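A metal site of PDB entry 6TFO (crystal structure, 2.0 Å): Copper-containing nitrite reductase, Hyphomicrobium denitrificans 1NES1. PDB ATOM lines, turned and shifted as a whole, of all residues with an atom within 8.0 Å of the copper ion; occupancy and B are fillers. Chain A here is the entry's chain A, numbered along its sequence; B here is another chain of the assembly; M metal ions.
The side-chain carboxylate (OE2) of Glu 76 is in hydrogen-bond range of a ring nitrogen (NE2) of His 80.
O of His 80 lies within hydrogen-bond range of N of Val 94.
SG of Cys 117 sits close to N of Leu 119 (3.5 Å).
SG of Cys 117 lies close to N of Asp 81 (3.7 Å).
N of Cys 117 sits at hydrogen-bond distance from OH of Tyr 45, 2.9 Å away.
O of Gln 79 sits close to ND1 of His 122 (3.2 Å).
The backbone NH (N) of Met 127 sits at hydrogen-bond distance from the backbone carbonyl oxygen (O) of Met 43 (3.0 Å).
Gln 79 touches the copper ion (O to CU, 3.2 Å).
The nearest printed residue that does not touch the copper ion is Leu 119 (4.3 Å).
The copper ion is bound by ND1 of His 80 (2.0 Å), SG of Cys 117 (2.2 Å), ND1 of His 122 (2.3 Å) and SD of Met 127 (2.6 Å).
The copper ion has four donor atoms within binding distance.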
ATOM      1  N   THR A  36      21.942 -32.496  -5.519  1.00  0.00           N
ATOM      2  CA  THR A  36      20.927 -32.524  -4.454  1.00  0.00           C
ATOM      3  C   THR A  36      20.818 -33.966  -3.958  1.00  0.00           C
ATOM      4  O   THR A  36      21.058 -34.909  -4.761  1.00  0.00           O
ATOM      5  CB  THR A  36      19.564 -32.020  -4.935  1.00  0.00           C
ATOM      6  OG1 THR A  36      19.076 -32.941  -5.902  1.00  0.00           O
ATOM      7  CG2 THR A  36      19.668 -30.622  -5.506  1.00  0.00           C
ATOM      8  N   MET A  43      17.632 -33.075   3.677  1.00  0.00           N
ATOM      9  CA  MET A  43      17.694 -32.795   2.231  1.00  0.00           C
ATOM     10  C   MET A  43      18.728 -31.675   2.013  1.00  0.00           C
ATOM     11  O   MET A  43      18.521 -30.570   2.544  1.00  0.00           O
ATOM     12  CB  MET A  43      16.338 -32.359   1.689  1.00  0.00           C
ATOM     13  CG  MET A  43      16.245 -32.507   0.187  1.00  0.00           C
ATOM     14  SD  MET A  43      14.601 -32.253  -0.449  1.00  0.00           S
ATOM     15  CE  MET A  43      14.102 -30.809   0.474  1.00  0.00           C
ATOM     16  N   VAL A  44      19.811 -31.981   1.286  1.00  0.00           N
ATOM     17  CA  VAL A  44      21.021 -31.118   1.230  1.00  0.00           C
ATOM     18  C   VAL A  44      21.566 -31.003  -0.203  1.00  0.00           C
ATOM     19  O   VAL A  44      21.053 -31.656  -1.134  1.00  0.00           O
ATOM     20  CB  VAL A  44      22.116 -31.650   2.163  1.00  0.00           C
ATOM     21  CG1 VAL A  44      21.666 -31.628   3.606  1.00  0.00           C
ATOM     22  CG2 VAL A  44      22.594 -33.034   1.764  1.00  0.00           C
ATOM     23  N   TYR A  45      22.581 -30.148  -0.341  1.00  0.00           N
ATOM     24  CA  TYR A  45      23.488 -30.131  -1.509  1.00  0.00           C
ATOM     25  C   TYR A  45      24.677 -30.995  -1.119  1.00  0.00           C
ATOM     26  O   TYR A  45      25.107 -30.941   0.062  1.00  0.00           O
ATOM     27  CB  TYR A  45      23.898 -28.693  -1.838  1.00  0.00           C
ATOM     28  CG  TYR A  45      22.790 -27.746  -2.212  1.00  0.00           C
ATOM     29  CD1 TYR A  45      22.248 -27.744  -3.501  1.00  0.00           C
ATOM     30  CD2 TYR A  45      22.353 -26.771  -1.331  1.00  0.00           C
ATOM     31  CE1 TYR A  45      21.269 -26.823  -3.871  1.00  0.00           C
ATOM     32  CE2 TYR A  45      21.384 -25.845  -1.693  1.00  0.00           C
ATOM     33  CZ  TYR A  45      20.845 -25.865  -2.971  1.00  0.00           C
ATOM     34  OH  TYR A  45      19.901 -24.951  -3.320  1.00  0.00           O
ATOM     35  N   LEU A  72      24.359 -27.064 -10.881  1.00  0.00           N
ATOM     36  CA  LEU A  72      23.383 -27.811 -10.042  1.00  0.00           C
ATOM     37  C   LEU A  72      22.887 -29.033 -10.819  1.00  0.00           C
ATOM     38  O   LEU A  72      22.369 -28.856 -11.912  1.00  0.00           O
ATOM     39  CB  LEU A  72      22.200 -26.937  -9.634  1.00  0.00           C
ATOM     40  CG  LEU A  72      21.213 -27.580  -8.668  1.00  0.00           C
ATOM     41  CD1 LEU A  72      21.910 -27.991  -7.393  1.00  0.00           C
ATOM     42  CD2 LEU A  72      20.073 -26.645  -8.343  1.00  0.00           C
ATOM     43  N   ASN A  74      20.373 -32.450 -10.172  1.00  0.00           N
ATOM     44  CA  ASN A  74      19.303 -33.104  -9.377  1.00  0.00           C
ATOM     45  C   ASN A  74      19.728 -34.547  -9.080  1.00  0.00           C
ATOM     46  O   ASN A  74      19.945 -35.287 -10.041  1.00  0.00           O
ATOM     47  CB  ASN A  74      17.981 -33.051 -10.132  1.00  0.00           C
ATOM     48  CG  ASN A  74      16.803 -33.457  -9.284  1.00  0.00           C
ATOM     49  OD1 ASN A  74      16.875 -34.454  -8.578  1.00  0.00           O
ATOM     50  ND2 ASN A  74      15.732 -32.701  -9.355  1.00  0.00           N
ATOM     51  N   GLU A  76      18.064 -36.812  -6.454  1.00  0.00           N
ATOM     52  CA  GLU A  76      17.038 -37.729  -5.881  1.00  0.00           C
ATOM     53  C   GLU A  76      15.644 -37.510  -6.498  1.00  0.00           C
ATOM     54  O   GLU A  76      14.818 -38.434  -6.390  1.00  0.00           O
ATOM     55  CB  GLU A  76      17.021 -37.594  -4.367  1.00  0.00           C
ATOM     56  CG  GLU A  76      16.146 -36.473  -3.836  1.00  0.00           C
ATOM     57  CD  GLU A  76      16.484 -35.086  -4.336  1.00  0.00           C
ATOM     58  OE1 GLU A  76      17.660 -34.728  -4.314  1.00  0.00           O
ATOM     59  OE2 GLU A  76      15.553 -34.379  -4.731  1.00  0.00           O
ATOM     60  N   ALA A  78      13.386 -34.529  -6.468  1.00  0.00           N
ATOM     61  CA  ALA A  78      12.473 -33.438  -6.041  1.00  0.00           C
ATOM     62  C   ALA A  78      12.794 -32.184  -6.871  1.00  0.00           C
ATOM     63  O   ALA A  78      13.784 -32.223  -7.590  1.00  0.00           O
ATOM     64  CB  ALA A  78      12.582 -33.200  -4.557  1.00  0.00           C
ATOM     65  N   GLN A  79      11.985 -31.128  -6.784  1.00  0.00           N
ATOM     66  CA  GLN A  79      12.265 -29.833  -7.468  1.00  0.00           C
ATOM     67  C   GLN A  79      13.285 -29.075  -6.626  1.00  0.00           C
ATOM     68  O   GLN A  79      13.142 -29.055  -5.406  1.00  0.00           O
ATOM     69  CB  GLN A  79      11.010 -29.015  -7.695  1.00  0.00           C
ATOM     70  CG  GLN A  79      10.048 -29.684  -8.657  1.00  0.00           C
ATOM     71  CD  GLN A  79       9.001 -28.705  -9.142  1.00  0.00           C
ATOM     72  OE1 GLN A  79       8.537 -27.861  -8.383  1.00  0.00           O
ATOM     73  NE2 GLN A  79       8.647 -28.817 -10.403  1.00  0.00           N
ATOM     74  N   HIS A  80      14.288 -28.501  -7.297  1.00  0.00           N
ATOM     75  CA  HIS A  80      15.419 -27.773  -6.671  1.00  0.00           C
ATOM     76  C   HIS A  80      15.913 -26.638  -7.563  1.00  0.00           C
ATOM     77  O   HIS A  80      15.878 -26.761  -8.812  1.00  0.00           O
ATOM     78  CB  HIS A  80      16.603 -28.718  -6.356  1.00  0.00           C
ATOM     79  CG  HIS A  80      16.264 -29.890  -5.497  1.00  0.00           C
ATOM     80  ND1 HIS A  80      15.933 -29.743  -4.176  1.00  0.00           N
ATOM     81  CD2 HIS A  80      16.201 -31.205  -5.781  1.00  0.00           C
ATOM     82  CE1 HIS A  80      15.695 -30.936  -3.674  1.00  0.00           C
ATOM     83  NE2 HIS A  80      15.831 -31.840  -4.646  1.00  0.00           N
ATOM     84  N   ASP A  81      16.367 -25.565  -6.915  1.00  0.00           N
ATOM     85  CA  ASP A  81      17.280 -24.570  -7.512  1.00  0.00           C
ATOM     86  C   ASP A  81      18.360 -24.255  -6.470  1.00  0.00           C
ATOM     87  O   ASP A  81      18.381 -24.890  -5.392  1.00  0.00           O
ATOM     88  CB  ASP A  81      16.503 -23.355  -8.002  1.00  0.00           C
ATOM     89  CG  ASP A  81      15.804 -22.609  -6.884  1.00  0.00           C
ATOM     90  OD1 ASP A  81      16.210 -22.809  -5.734  1.00  0.00           O
ATOM     91  OD2 ASP A  81      14.896 -21.838  -7.169  1.00  0.00           O
ATOM     92  N   ALA A  82      19.289 -23.377  -6.822  1.00  0.00           N
ATOM     93  CA  ALA A  82      20.244 -22.742  -5.915  1.00  0.00           C
ATOM     94  C   ALA A  82      20.132 -21.242  -6.138  1.00  0.00           C
ATOM     95  O   ALA A  82      20.079 -20.822  -7.313  1.00  0.00           O
ATOM     96  CB  ALA A  82      21.633 -23.278  -6.157  1.00  0.00           C
ATOM     97  N   VAL A  94      15.426 -27.470 -11.378  1.00  0.00           N
ATOM     98  CA  VAL A  94      15.680 -28.814 -11.966  1.00  0.00           C
ATOM     99  C   VAL A  94      14.729 -29.829 -11.307  1.00  0.00           C
ATOM    100  O   VAL A  94      14.718 -29.893 -10.059  1.00  0.00           O
ATOM    101  CB  VAL A  94      17.163 -29.193 -11.816  1.00  0.00           C
ATOM    102  CG1 VAL A  94      18.015 -28.461 -12.834  1.00  0.00           C
ATOM    103  CG2 VAL A  94      17.698 -28.988 -10.401  1.00  0.00           C
ATOM    104  N   TYR A 116      21.020 -21.378  -1.348  1.00  0.00           N
ATOM    105  CA  TYR A 116      19.876 -22.119  -0.807  1.00  0.00           C
ATOM    106  C   TYR A 116      18.887 -22.465  -1.916  1.00  0.00           C
ATOM    107  O   TYR A 116      18.901 -21.846  -2.979  1.00  0.00           O
ATOM    108  CB  TYR A 116      19.225 -21.277   0.297  1.00  0.00           C
ATOM    109  CG  TYR A 116      18.513 -20.067  -0.210  1.00  0.00           C
ATOM    110  CD1 TYR A 116      17.195 -20.134  -0.619  1.00  0.00           C
ATOM    111  CD2 TYR A 116      19.169 -18.856  -0.324  1.00  0.00           C
ATOM    112  CE1 TYR A 116      16.525 -19.027  -1.095  1.00  0.00           C
ATOM    113  CE2 TYR A 116      18.523 -17.725  -0.786  1.00  0.00           C
ATOM    114  CZ  TYR A 116      17.198 -17.811  -1.186  1.00  0.00           C
ATOM    115  OH  TYR A 116      16.549 -16.719  -1.678  1.00  0.00           O
ATOM    116  N   CYS A 117      18.024 -23.442  -1.640  1.00  0.00           N
ATOM    117  CA  CYS A 117      16.898 -23.845  -2.517  1.00  0.00           C
ATOM    118  C   CYS A 117      15.674 -23.029  -2.130  1.00  0.00           C
ATOM    119  O   CYS A 117      15.379 -22.927  -0.934  1.00  0.00           O
ATOM    120  CB  CYS A 117      16.627 -25.328  -2.404  1.00  0.00           C
ATOM    121  SG  CYS A 117      15.251 -25.864  -3.442  1.00  0.00           S
ATOM    122  N   SER A 118      14.988 -22.448  -3.102  1.00  0.00           N
ATOM    123  CA  SER A 118      13.822 -21.560  -2.861  1.00  0.00           C
ATOM    124  C   SER A 118      12.522 -22.375  -2.922  1.00  0.00           C
ATOM    125  O   SER A 118      11.476 -21.760  -2.671  1.00  0.00           O
ATOM    126  CB  SER A 118      13.777 -20.447  -3.863  1.00  0.00           C
ATOM    127  OG  SER A 118      13.491 -20.976  -5.137  1.00  0.00           O
ATOM    128  N   LEU A 119      12.564 -23.659  -3.273  1.00  0.00           N
ATOM    129  CA  LEU A 119      11.329 -24.486  -3.358  1.00  0.00           C
ATOM    130  C   LEU A 119      10.688 -24.558  -1.969  1.00  0.00           C
ATOM    131  O   LEU A 119      11.383 -24.556  -0.960  1.00  0.00           O
ATOM    132  CB  LEU A 119      11.632 -25.878  -3.937  1.00  0.00           C
ATOM    133  CG  LEU A 119      11.560 -26.006  -5.467  1.00  0.00           C
ATOM    134  CD1 LEU A 119      10.195 -25.559  -6.006  1.00  0.00           C
ATOM    135  CD2 LEU A 119      12.677 -25.227  -6.135  1.00  0.00           C
ATOM    136  N   PRO A 120       9.339 -24.613  -1.856  1.00  0.00           N
ATOM    137  CA  PRO A 120       8.686 -24.551  -0.555  1.00  0.00           C
ATOM    138  C   PRO A 120       9.262 -25.555   0.448  1.00  0.00           C
ATOM    139  O   PRO A 120       9.286 -26.752   0.183  1.00  0.00           O
ATOM    140  CB  PRO A 120       7.217 -24.863  -0.880  1.00  0.00           C
ATOM    141  CG  PRO A 120       7.049 -24.412  -2.326  1.00  0.00           C
ATOM    142  CD  PRO A 120       8.386 -24.727  -2.972  1.00  0.00           C
ATOM    143  N   GLY A 121       9.806 -25.017   1.554  1.00  0.00           N
ATOM    144  CA  GLY A 121      10.290 -25.806   2.698  1.00  0.00           C
ATOM    145  C   GLY A 121      11.690 -26.375   2.514  1.00  0.00           C
ATOM    146  O   GLY A 121      12.244 -26.848   3.542  1.00  0.00           O
ATOM    147  N   HIS A 122      12.282 -26.344   1.312  1.00  0.00           N
ATOM    148  CA  HIS A 122      13.543 -27.100   1.023  1.00  0.00           C
ATOM    149  C   HIS A 122      14.693 -26.492   1.816  1.00  0.00           C
ATOM    150  O   HIS A 122      15.599 -27.241   2.235  1.00  0.00           O
ATOM    151  CB  HIS A 122      13.804 -27.174  -0.480  1.00  0.00           C
ATOM    152  CG  HIS A 122      12.937 -28.172  -1.180  1.00  0.00           C
ATOM    153  ND1 HIS A 122      13.395 -28.949  -2.232  1.00  0.00           N
ATOM    154  CD2 HIS A 122      11.656 -28.551  -0.971  1.00  0.00           C
ATOM    155  CE1 HIS A 122      12.427 -29.744  -2.661  1.00  0.00           C
ATOM    156  NE2 HIS A 122      11.343 -29.508  -1.909  1.00  0.00           N
ATOM    157  N   ARG A 123      14.670 -25.180   2.063  1.00  0.00           N
ATOM    158  CA  ARG A 123      15.757 -24.495   2.797  1.00  0.00           C
ATOM    159  C   ARG A 123      15.692 -24.941   4.260  1.00  0.00           C
ATOM    160  O   ARG A 123      16.744 -25.378   4.801  1.00  0.00           O
ATOM    161  CB  ARG A 123      15.622 -22.973   2.661  1.00  0.00           C
ATOM    162  CG  ARG A 123      16.790 -22.187   3.226  1.00  0.00           C
ATOM    163  CD  ARG A 123      16.597 -20.700   3.027  1.00  0.00           C
ATOM    164  NE  ARG A 123      17.827 -19.975   3.322  1.00  0.00           N
ATOM    165  CZ  ARG A 123      18.052 -18.689   3.043  1.00  0.00           C
ATOM    166  NH1 ARG A 123      19.222 -18.151   3.356  1.00  0.00           N
ATOM    167  NH2 ARG A 123      17.135 -17.971   2.438  1.00  0.00           N
ATOM    168  N   ALA A 125      14.404 -27.634   5.318  1.00  0.00           N
ATOM    169  CA  ALA A 125      14.688 -29.102   5.304  1.00  0.00           C
ATOM    170  C   ALA A 125      16.192 -29.390   5.255  1.00  0.00           C
ATOM    171  O   ALA A 125      16.543 -30.554   5.432  1.00  0.00           O
ATOM    172  CB  ALA A 125      13.988 -29.738   4.129  1.00  0.00           C
ATOM    173  N   MET A 127      18.523 -27.544   2.718  1.00  0.00           N
ATOM    174  CA  MET A 127      19.177 -27.138   1.456  1.00  0.00           C
ATOM    175  C   MET A 127      19.713 -25.708   1.577  1.00  0.00           C
ATOM    176  O   MET A 127      19.037 -24.748   1.158  1.00  0.00           O
ATOM    177  CB  MET A 127      18.205 -27.261   0.272  1.00  0.00           C
ATOM    178  CG  MET A 127      17.812 -28.698   0.016  1.00  0.00           C
ATOM    179  SD  MET A 127      17.162 -28.919  -1.627  1.00  0.00           S
ATOM    180  CE  MET A 127      18.696 -29.230  -2.509  1.00  0.00           C
ATOM    181  N   ALA B 125       7.101 -29.245   1.501  1.00  0.00           N
ATOM    182  CA  ALA B 125       7.829 -30.019   0.465  1.00  0.00           C
ATOM    183  C   ALA B 125       6.957 -31.130  -0.139  1.00  0.00           C
ATOM    184  O   ALA B 125       7.390 -31.713  -1.145  1.00  0.00           O
ATOM    185  CB  ALA B 125       9.091 -30.580   1.061  1.00  0.00           C
HETATM  186 CU    CU M   1      15.250 -28.094  -3.236  1.00  0.00          CU
